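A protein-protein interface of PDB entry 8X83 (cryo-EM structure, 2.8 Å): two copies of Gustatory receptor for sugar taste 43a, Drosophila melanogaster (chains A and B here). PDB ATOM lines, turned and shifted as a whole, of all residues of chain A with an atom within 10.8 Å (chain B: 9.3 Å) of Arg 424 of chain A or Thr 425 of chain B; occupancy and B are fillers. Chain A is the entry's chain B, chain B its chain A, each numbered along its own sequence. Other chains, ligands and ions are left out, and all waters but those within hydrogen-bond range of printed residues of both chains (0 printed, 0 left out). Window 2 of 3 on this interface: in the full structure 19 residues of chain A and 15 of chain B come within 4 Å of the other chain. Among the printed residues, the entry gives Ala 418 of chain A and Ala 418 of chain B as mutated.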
ATOM      1  N   THR A  75      -2.191  17.995  -6.822  1.00  0.00           N
ATOM      2  CA  THR A  75      -3.185  18.565  -5.921  1.00  0.00           C
ATOM      3  C   THR A  75      -2.601  19.739  -5.145  1.00  0.00           C
ATOM      4  O   THR A  75      -3.222  20.804  -5.044  1.00  0.00           O
ATOM      5  CB  THR A  75      -3.699  17.492  -4.962  1.00  0.00           C
ATOM      6  OG1 THR A  75      -3.999  16.295  -5.690  1.00  0.00           O
ATOM      7  CG2 THR A  75      -4.951  17.971  -4.248  1.00  0.00           C
ATOM      8  N   TYR A 312      -8.040  21.531   4.039  1.00  0.00           N
ATOM      9  CA  TYR A 312      -7.513  20.365   3.337  1.00  0.00           C
ATOM     10  C   TYR A 312      -6.075  20.075   3.753  1.00  0.00           C
ATOM     11  O   TYR A 312      -5.711  18.921   4.008  1.00  0.00           O
ATOM     12  CB  TYR A 312      -7.612  20.590   1.828  1.00  0.00           C
ATOM     13  CG  TYR A 312      -6.896  19.562   0.985  1.00  0.00           C
ATOM     14  CD1 TYR A 312      -7.476  18.330   0.717  1.00  0.00           C
ATOM     15  CD2 TYR A 312      -5.651  19.832   0.435  1.00  0.00           C
ATOM     16  CE1 TYR A 312      -6.830  17.391  -0.061  1.00  0.00           C
ATOM     17  CE2 TYR A 312      -4.998  18.900  -0.347  1.00  0.00           C
ATOM     18  CZ  TYR A 312      -5.593  17.683  -0.592  1.00  0.00           C
ATOM     19  OH  TYR A 312      -4.947  16.748  -1.367  1.00  0.00           O
ATOM     20  N   PHE A 315      -6.059  18.651   7.242  1.00  0.00           N
ATOM     21  CA  PHE A 315      -6.471  17.252   7.254  1.00  0.00           C
ATOM     22  C   PHE A 315      -5.347  16.352   6.753  1.00  0.00           C
ATOM     23  O   PHE A 315      -5.113  15.268   7.302  1.00  0.00           O
ATOM     24  CB  PHE A 315      -7.741  17.090   6.415  1.00  0.00           C
ATOM     25  CG  PHE A 315      -7.932  15.718   5.836  1.00  0.00           C
ATOM     26  CD1 PHE A 315      -8.732  14.791   6.480  1.00  0.00           C
ATOM     27  CD2 PHE A 315      -7.344  15.365   4.634  1.00  0.00           C
ATOM     28  CE1 PHE A 315      -8.923  13.532   5.948  1.00  0.00           C
ATOM     29  CE2 PHE A 315      -7.530  14.107   4.099  1.00  0.00           C
ATOM     30  CZ  PHE A 315      -8.323  13.192   4.756  1.00  0.00           C
ATOM     31  N   LEU A 316      -4.636  16.790   5.710  1.00  0.00           N
ATOM     32  CA  LEU A 316      -3.487  16.028   5.229  1.00  0.00           C
ATOM     33  C   LEU A 316      -2.432  15.875   6.318  1.00  0.00           C
ATOM     34  O   LEU A 316      -1.942  14.766   6.571  1.00  0.00           O
ATOM     35  CB  LEU A 316      -2.885  16.712   4.005  1.00  0.00           C
ATOM     36  CG  LEU A 316      -3.330  16.173   2.648  1.00  0.00           C
ATOM     37  CD1 LEU A 316      -4.726  16.655   2.348  1.00  0.00           C
ATOM     38  CD2 LEU A 316      -2.370  16.615   1.555  1.00  0.00           C
ATOM     39  N   GLU A 317      -2.066  16.981   6.970  1.00  0.00           N
ATOM     40  CA  GLU A 317      -1.051  16.921   8.017  1.00  0.00           C
ATOM     41  C   GLU A 317      -1.539  16.113   9.213  1.00  0.00           C
ATOM     42  O   GLU A 317      -0.736  15.516   9.938  1.00  0.00           O
ATOM     43  CB  GLU A 317      -0.660  18.335   8.446  1.00  0.00           C
ATOM     44  CG  GLU A 317       0.576  18.404   9.326  1.00  0.00           C
ATOM     45  CD  GLU A 317       1.859  18.078   8.583  1.00  0.00           C
ATOM     46  OE1 GLU A 317       1.784  17.639   7.416  1.00  0.00           O
ATOM     47  OE2 GLU A 317       2.947  18.263   9.169  1.00  0.00           O
ATOM     48  N   LEU A 318      -2.854  16.087   9.436  1.00  0.00           N
ATOM     49  CA  LEU A 318      -3.400  15.328  10.554  1.00  0.00           C
ATOM     50  C   LEU A 318      -3.362  13.835  10.263  1.00  0.00           C
ATOM     51  O   LEU A 318      -3.167  13.021  11.174  1.00  0.00           O
ATOM     52  CB  LEU A 318      -4.826  15.800  10.845  1.00  0.00           C
ATOM     53  CG  LEU A 318      -5.373  15.708  12.272  1.00  0.00           C
ATOM     54  CD1 LEU A 318      -4.415  16.292  13.302  1.00  0.00           C
ATOM     55  CD2 LEU A 318      -6.707  16.433  12.338  1.00  0.00           C
ATOM     56  N   LEU A 319      -3.560  13.453   9.000  1.00  0.00           N
ATOM     57  CA  LEU A 319      -3.359  12.057   8.624  1.00  0.00           C
ATOM     58  C   LEU A 319      -1.889  11.672   8.727  1.00  0.00           C
ATOM     59  O   LEU A 319      -1.540  10.671   9.364  1.00  0.00           O
ATOM     60  CB  LEU A 319      -3.874  11.802   7.207  1.00  0.00           C
ATOM     61  CG  LEU A 319      -5.370  11.980   6.950  1.00  0.00           C
ATOM     62  CD1 LEU A 319      -5.679  11.568   5.521  1.00  0.00           C
ATOM     63  CD2 LEU A 319      -6.206  11.194   7.949  1.00  0.00           C
ATOM     64  N   SER A 320      -1.007  12.461   8.108  1.00  0.00           N
ATOM     65  CA  SER A 320       0.411  12.118   8.112  1.00  0.00           C
ATOM     66  C   SER A 320       1.055  12.427   9.457  1.00  0.00           C
ATOM     67  O   SER A 320       1.934  11.688   9.915  1.00  0.00           O
ATOM     68  CB  SER A 320       1.129  12.866   6.993  1.00  0.00           C
ATOM     69  OG  SER A 320       0.563  12.560   5.731  1.00  0.00           O
ATOM     70  N   LEU A 416     -14.623  20.889   0.272  1.00  0.00           N
ATOM     71  CA  LEU A 416     -13.625  20.252   1.132  1.00  0.00           C
ATOM     72  C   LEU A 416     -13.872  18.760   1.226  1.00  0.00           C
ATOM     73  O   LEU A 416     -12.966  17.988   0.981  1.00  0.00           O
ATOM     74  CB  LEU A 416     -13.618  20.869   2.527  1.00  0.00           C
ATOM     75  CG  LEU A 416     -12.323  20.907   3.334  1.00  0.00           C
ATOM     76  CD1 LEU A 416     -12.673  20.895   4.812  1.00  0.00           C
ATOM     77  CD2 LEU A 416     -11.408  19.746   3.002  1.00  0.00           C
ATOM     78  N   VAL A 417     -15.117  18.344   1.452  1.00  0.00           N
ATOM     79  CA  VAL A 417     -15.425  16.916   1.551  1.00  0.00           C
ATOM     80  C   VAL A 417     -15.067  16.229   0.239  1.00  0.00           C
ATOM     81  O   VAL A 417     -14.352  15.223   0.227  1.00  0.00           O
ATOM     82  CB  VAL A 417     -16.919  16.691   1.830  1.00  0.00           C
ATOM     83  CG1 VAL A 417     -17.344  15.305   1.373  1.00  0.00           C
ATOM     84  CG2 VAL A 417     -17.224  16.904   3.302  1.00  0.00           C
ATOM     85  N   ALA A 418     -15.377  16.848  -1.110  1.00  0.00           N
ATOM     86  CA  ALA A 418     -14.969  16.359  -2.421  1.00  0.00           C
ATOM     87  C   ALA A 418     -13.455  16.258  -2.509  1.00  0.00           C
ATOM     88  O   ALA A 418     -12.914  15.206  -2.874  1.00  0.00           O
ATOM     89  CB  ALA A 418     -15.512  17.273  -3.517  1.00  0.00           C
ATOM     90  N   LEU A 419     -12.899  17.285  -1.902  1.00  0.00           N
ATOM     91  CA  LEU A 419     -11.449  17.291  -1.994  1.00  0.00           C
ATOM     92  C   LEU A 419     -10.868  16.109  -1.207  1.00  0.00           C
ATOM     93  O   LEU A 419      -9.892  15.498  -1.634  1.00  0.00           O
ATOM     94  CB  LEU A 419     -10.892  18.614  -1.469  1.00  0.00           C
ATOM     95  CG  LEU A 419      -9.857  19.293  -2.365  1.00  0.00           C
ATOM     96  CD1 LEU A 419      -9.285  20.523  -1.678  1.00  0.00           C
ATOM     97  CD2 LEU A 419      -8.754  18.326  -2.761  1.00  0.00           C
ATOM     98  N   ILE A 420     -11.460  15.803  -0.052  1.00  0.00           N
ATOM     99  CA  ILE A 420     -11.004  14.707   0.781  1.00  0.00           C
ATOM    100  C   ILE A 420     -11.252  13.422   0.036  1.00  0.00           C
ATOM    101  O   ILE A 420     -10.394  12.542   0.000  1.00  0.00           O
ATOM    102  CB  ILE A 420     -11.758  14.645   2.121  1.00  0.00           C
ATOM    103  CG1 ILE A 420     -11.491  15.904   2.940  1.00  0.00           C
ATOM    104  CG2 ILE A 420     -11.335  13.416   2.908  1.00  0.00           C
ATOM    105  CD1 ILE A 420     -10.027  16.267   3.040  1.00  0.00           C
ATOM    106  N   GLN A 421     -12.430  13.305  -0.565  1.00  0.00           N
ATOM    107  CA  GLN A 421     -12.737  12.096  -1.313  1.00  0.00           C
ATOM    108  C   GLN A 421     -11.734  11.932  -2.452  1.00  0.00           C
ATOM    109  O   GLN A 421     -11.330  10.820  -2.781  1.00  0.00           O
ATOM    110  CB  GLN A 421     -14.153  12.185  -1.882  1.00  0.00           C
ATOM    111  CG  GLN A 421     -14.611  10.936  -2.609  1.00  0.00           C
ATOM    112  CD  GLN A 421     -15.221   9.914  -1.675  1.00  0.00           C
ATOM    113  OE1 GLN A 421     -14.830   8.749  -1.669  1.00  0.00           O
ATOM    114  NE2 GLN A 421     -16.187  10.350  -0.875  1.00  0.00           N
ATOM    115  N   PHE A 422     -11.340  13.050  -3.053  1.00  0.00           N
ATOM    116  CA  PHE A 422     -10.386  13.042  -4.151  1.00  0.00           C
ATOM    117  C   PHE A 422      -9.031  12.492  -3.715  1.00  0.00           C
ATOM    118  O   PHE A 422      -8.320  11.888  -4.513  1.00  0.00           O
ATOM    119  CB  PHE A 422     -10.221  14.439  -4.743  1.00  0.00           C
ATOM    120  CG  PHE A 422      -9.839  14.427  -6.190  1.00  0.00           C
ATOM    121  CD1 PHE A 422      -8.577  14.819  -6.600  1.00  0.00           C
ATOM    122  CD2 PHE A 422     -10.743  13.995  -7.142  1.00  0.00           C
ATOM    123  CE1 PHE A 422      -8.230  14.795  -7.938  1.00  0.00           C
ATOM    124  CE2 PHE A 422     -10.405  13.966  -8.479  1.00  0.00           C
ATOM    125  CZ  PHE A 422      -9.146  14.367  -8.879  1.00  0.00           C
ATOM    126  N   GLN A 423      -8.656  12.735  -2.464  1.00  0.00           N
ATOM    127  CA  GLN A 423      -7.389  12.239  -1.941  1.00  0.00           C
ATOM    128  C   GLN A 423      -7.417  10.717  -1.915  1.00  0.00           C
ATOM    129  O   GLN A 423      -6.451  10.061  -2.300  1.00  0.00           O
ATOM    130  CB  GLN A 423      -7.138  12.788  -0.535  1.00  0.00           C
ATOM    131  CG  GLN A 423      -5.891  12.243   0.141  1.00  0.00           C
ATOM    132  CD  GLN A 423      -4.618  12.926  -0.324  1.00  0.00           C
ATOM    133  OE1 GLN A 423      -3.562  12.773   0.290  1.00  0.00           O
ATOM    134  NE2 GLN A 423      -4.710  13.685  -1.412  1.00  0.00           N
ATOM    135  N   ARG A 424      -8.532  10.160  -1.454  1.00  0.00           N
ATOM    136  CA  ARG A 424      -8.699   8.714  -1.393  1.00  0.00           C
ATOM    137  C   ARG A 424      -8.662   8.113  -2.795  1.00  0.00           C
ATOM    138  O   ARG A 424      -8.060   7.064  -3.018  1.00  0.00           O
ATOM    139  CB  ARG A 424     -10.025   8.361  -0.716  1.00  0.00           C
ATOM    140  CG  ARG A 424      -9.950   8.293   0.799  1.00  0.00           C
ATOM    141  CD  ARG A 424      -9.386   9.575   1.387  1.00  0.00           C
ATOM    142  NE  ARG A 424      -9.035   9.420   2.795  1.00  0.00           N
ATOM    143  CZ  ARG A 424      -7.876   8.935   3.228  1.00  0.00           C
ATOM    144  NH1 ARG A 424      -7.642   8.829   4.529  1.00  0.00           N
ATOM    145  NH2 ARG A 424      -6.948   8.554   2.361  1.00  0.00           N
ATOM    146  N   THR A 425      -9.308   8.794  -3.736  1.00  0.00           N
ATOM    147  CA  THR A 425      -9.365   8.335  -5.118  1.00  0.00           C
ATOM    148  C   THR A 425      -8.088   8.698  -5.864  1.00  0.00           C
ATOM    149  O   THR A 425      -7.109   7.956  -5.827  1.00  0.00           O
ATOM    150  CB  THR A 425     -10.568   8.951  -5.857  1.00  0.00           C
ATOM    151  OG1 THR A 425     -11.777   8.622  -5.164  1.00  0.00           O
ATOM    152  CG2 THR A 425     -10.646   8.436  -7.287  1.00  0.00           C
ATOM    153  N   ALA B  74     -11.174   5.973  12.672  1.00  0.00           N
ATOM    154  CA  ALA B  74     -11.036   7.400  12.399  1.00  0.00           C
ATOM    155  C   ALA B  74     -12.381   8.019  12.049  1.00  0.00           C
ATOM    156  O   ALA B  74     -12.733   9.089  12.560  1.00  0.00           O
ATOM    157  CB  ALA B  74     -10.031   7.623  11.270  1.00  0.00           C
ATOM    158  N   THR B  75     -13.155   7.356  11.189  1.00  0.00           N
ATOM    159  CA  THR B  75     -14.485   7.852  10.860  1.00  0.00           C
ATOM    160  C   THR B  75     -15.375   7.875  12.096  1.00  0.00           C
ATOM    161  O   THR B  75     -16.060   8.869  12.367  1.00  0.00           O
ATOM    162  CB  THR B  75     -15.111   6.988   9.765  1.00  0.00           C
ATOM    163  OG1 THR B  75     -14.156   6.762   8.721  1.00  0.00           O
ATOM    164  CG2 THR B  75     -16.337   7.670   9.183  1.00  0.00           C
ATOM    165  N   VAL B 417     -24.944  11.013   2.060  1.00  0.00           N
ATOM    166  CA  VAL B 417     -24.625  10.231   0.865  1.00  0.00           C
ATOM    167  C   VAL B 417     -23.118  10.237   0.643  1.00  0.00           C
ATOM    168  O   VAL B 417     -22.499   9.180   0.482  1.00  0.00           O
ATOM    169  CB  VAL B 417     -25.305  10.821  -0.380  1.00  0.00           C
ATOM    170  CG1 VAL B 417     -24.562  10.412  -1.640  1.00  0.00           C
ATOM    171  CG2 VAL B 417     -26.764  10.402  -0.439  1.00  0.00           C
ATOM    172  N   ALA B 418     -22.278  11.486   0.819  1.00  0.00           N
ATOM    173  CA  ALA B 418     -20.825  11.589   0.769  1.00  0.00           C
ATOM    174  C   ALA B 418     -20.186  10.682   1.808  1.00  0.00           C
ATOM    175  O   ALA B 418     -19.306   9.876   1.485  1.00  0.00           O
ATOM    176  CB  ALA B 418     -20.392  13.038   0.978  1.00  0.00           C
ATOM    177  N   LEU B 419     -20.887  10.711   2.922  1.00  0.00           N
ATOM    178  CA  LEU B 419     -20.306   9.913   3.988  1.00  0.00           C
ATOM    179  C   LEU B 419     -20.362   8.425   3.619  1.00  0.00           C
ATOM    180  O   LEU B 419     -19.434   7.675   3.913  1.00  0.00           O
ATOM    181  CB  LEU B 419     -21.041  10.172   5.302  1.00  0.00           C
ATOM    182  CG  LEU B 419     -20.147  10.447   6.512  1.00  0.00           C
ATOM    183  CD1 LEU B 419     -20.984  10.557   7.776  1.00  0.00           C
ATOM    184  CD2 LEU B 419     -19.074   9.381   6.657  1.00  0.00           C
ATOM    185  N   ILE B 420     -21.459   7.999   2.992  1.00  0.00           N
ATOM    186  CA  ILE B 420     -21.631   6.616   2.592  1.00  0.00           C
ATOM    187  C   ILE B 420     -20.611   6.310   1.526  1.00  0.00           C
ATOM    188  O   ILE B 420     -19.967   5.264   1.556  1.00  0.00           O
ATOM    189  CB  ILE B 420     -23.031   6.349   2.014  1.00  0.00           C
ATOM    190  CG1 ILE B 420     -24.099   6.589   3.077  1.00  0.00           C
ATOM    191  CG2 ILE B 420     -23.126   4.923   1.498  1.00  0.00           C
ATOM    192  CD1 ILE B 420     -23.807   5.915   4.398  1.00  0.00           C
ATOM    193  N   GLN B 421     -20.457   7.225   0.576  1.00  0.00           N
ATOM    194  CA  GLN B 421     -19.484   7.005  -0.482  1.00  0.00           C
ATOM    195  C   GLN B 421     -18.089   6.881   0.127  1.00  0.00           C
ATOM    196  O   GLN B 421     -17.265   6.097  -0.337  1.00  0.00           O
ATOM    197  CB  GLN B 421     -19.514   8.173  -1.466  1.00  0.00           C
ATOM    198  CG  GLN B 421     -18.596   8.005  -2.661  1.00  0.00           C
ATOM    199  CD  GLN B 421     -19.252   7.242  -3.791  1.00  0.00           C
ATOM    200  OE1 GLN B 421     -18.704   6.265  -4.297  1.00  0.00           O
ATOM    201  NE2 GLN B 421     -20.437   7.687  -4.192  1.00  0.00           N
ATOM    202  N   PHE B 422     -17.831   7.665   1.169  1.00  0.00           N
ATOM    203  CA  PHE B 422     -16.546   7.650   1.848  1.00  0.00           C
ATOM    204  C   PHE B 422     -16.256   6.288   2.473  1.00  0.00           C
ATOM    205  O   PHE B 422     -15.100   5.884   2.572  1.00  0.00           O
ATOM    206  CB  PHE B 422     -16.475   8.741   2.912  1.00  0.00           C
ATOM    207  CG  PHE B 422     -15.084   9.233   3.165  1.00  0.00           C
ATOM    208  CD1 PHE B 422     -14.430   8.949   4.351  1.00  0.00           C
ATOM    209  CD2 PHE B 422     -14.418   9.960   2.196  1.00  0.00           C
ATOM    210  CE1 PHE B 422     -13.142   9.399   4.572  1.00  0.00           C
ATOM    211  CE2 PHE B 422     -13.132  10.411   2.407  1.00  0.00           C
ATOM    212  CZ  PHE B 422     -12.491  10.130   3.597  1.00  0.00           C
ATOM    213  N   GLN B 423     -17.296   5.600   2.928  1.00  0.00           N
ATOM    214  CA  GLN B 423     -17.132   4.281   3.527  1.00  0.00           C
ATOM    215  C   GLN B 423     -16.618   3.311   2.471  1.00  0.00           C
ATOM    216  O   GLN B 423     -15.715   2.518   2.728  1.00  0.00           O
ATOM    217  CB  GLN B 423     -18.459   3.783   4.102  1.00  0.00           C
ATOM    218  CG  GLN B 423     -18.416   2.369   4.654  1.00  0.00           C
ATOM    219  CD  GLN B 423     -17.815   2.293   6.045  1.00  0.00           C
ATOM    220  OE1 GLN B 423     -17.926   1.271   6.723  1.00  0.00           O
ATOM    221  NE2 GLN B 423     -17.177   3.375   6.480  1.00  0.00           N
ATOM    222  N   ARG B 424     -17.207   3.376   1.281  1.00  0.00           N
ATOM    223  CA  ARG B 424     -16.799   2.519   0.176  1.00  0.00           C
ATOM    224  C   ARG B 424     -15.357   2.813  -0.224  1.00  0.00           C
ATOM    225  O   ARG B 424     -14.579   1.901  -0.500  1.00  0.00           O
ATOM    226  CB  ARG B 424     -17.721   2.731  -1.028  1.00  0.00           C
ATOM    227  CG  ARG B 424     -18.983   1.889  -1.000  1.00  0.00           C
ATOM    228  CD  ARG B 424     -19.756   2.085   0.293  1.00  0.00           C
ATOM    229  NE  ARG B 424     -20.799   1.078   0.463  1.00  0.00           N
ATOM    230  CZ  ARG B 424     -20.598  -0.126   0.988  1.00  0.00           C
ATOM    231  NH1 ARG B 424     -21.605  -0.979   1.105  1.00  0.00           N
ATOM    232  NH2 ARG B 424     -19.387  -0.480   1.398  1.00  0.00           N
ATOM    233  N   THR B 425     -15.009   4.095  -0.246  1.00  0.00           N
ATOM    234  CA  THR B 425     -13.667   4.525  -0.619  1.00  0.00           C
ATOM    235  C   THR B 425     -12.707   4.382   0.554  1.00  0.00           C
ATOM    236  O   THR B 425     -12.133   3.316   0.768  1.00  0.00           O
ATOM    237  CB  THR B 425     -13.666   5.991  -1.090  1.00  0.00           C
ATOM    238  OG1 THR B 425     -14.569   6.142  -2.191  1.00  0.00           O
ATOM    239  CG2 THR B 425     -12.269   6.421  -1.517  1.00  0.00           C
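The backbone carbonyl oxygen (O) of Gln 421 of chain B lies within hydrogen-bond range of the side-chain hydroxyl (OG1) of Thr 425 of chain B, at 3.3 Å. OG1 of Thr 425 of chain A sits at hydrogen-bond distance from O of Gln 421 of chain A.
The side-chain amide oxygen (OE1) of Gln 421 of chain A lies within hydrogen-bond range of the side-chain hydroxyl (OG1) of Thr 425 of chain B, 2.7 Å away.
Among the printed residues, pairs that only touch across the chains: Val 417 of chain A with Ala 418 of chain B, Ile 420 of chain A with Phe 422 of chain B, Gln 421 of chain A with Ala 418 of chain B, Gln 421 of chain A with Gln 421 of chain B, Gln 421 of chain A with Phe 422 of chain B, Arg 424 of chain A with Phe 422 of chain B and Arg 424 of chain A with Thr 425 of chain B.
Hydrophobic or aromatic side chains of chain B within 4 Å of the printed part of chain A: Ala 418 and Phe 422. Of the 18 printed residues of chain A, 4 touch a printed residue of chain B. Hydrophobic or aromatic side chains of chain A within 4 Å of the printed part of chain B: Val 417 and Ile 420. Among the printed residues, 8 pairs touch across the chains. Among the printed residues, no Asp or Glu carboxylate lies within 4 Å of a Lys or Arg side-chain nitrogen of the other chain.
Val 417 of chain A touches Ala 418 of chain B, but with the chains exchanged Ala 418 of chain A does not touch Val 417 of chain B (10.3 Å). Ile 420 of chain A touches Phe 422 of chain B, but with the chains exchanged Phe 422 of chain A does not touch Ile 420 of chain B (12.3 Å). Gln 421 of chain A touches Ala 418 of chain B, but with the chains exchanged Ala 418 of chain A does not touch Gln 421 of chain B (9.1 Å). Arg 424 of chain A touches Thr 425 of chain B, but with the chains exchanged Thr 425 of chain A does not touch Arg 424 of chain B (8.4 Å). Positions printed for both chains: 75, 417, 418, 419, 420, 421, 422, 423, 424 and 425. Of the 8 pairs that touch across the chains among the printed residues, 1 has its exchanged pair printed and touching as well.
Arg 424 of chain A touches just these residues of chain B: Phe 422 and Thr 425. Thr 425 of chain B touches just these residues of chain A: Gln 421 (2.7 Å) and Arg 424 (3.1 Å). No residue of chain B comes within 4 Å of Thr 425 of chain A. Gln 421 of chain B touches one residue of chain A. Of the printed residues of chain B, Val 417 of chain A touches Ala 418. Of the printed residues of chain B, Ile 420 of chain A touches Phe 422. Of the printed residues of chain A, Ala 418 of chain B touches Val 417 and Gln 421. Glu 317 of chain A touches none of the printed residues of chain B. Ser 320 of chain A touches none of the printed residues of chain B. The nearest residue of chain B that does not touch Arg 424 of chain A is Ala 74 of chain B (7.3 Å). The nearest residue of chain A that does not touch Thr 425 of chain B is Thr 425 of chain A (4.3 Å).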
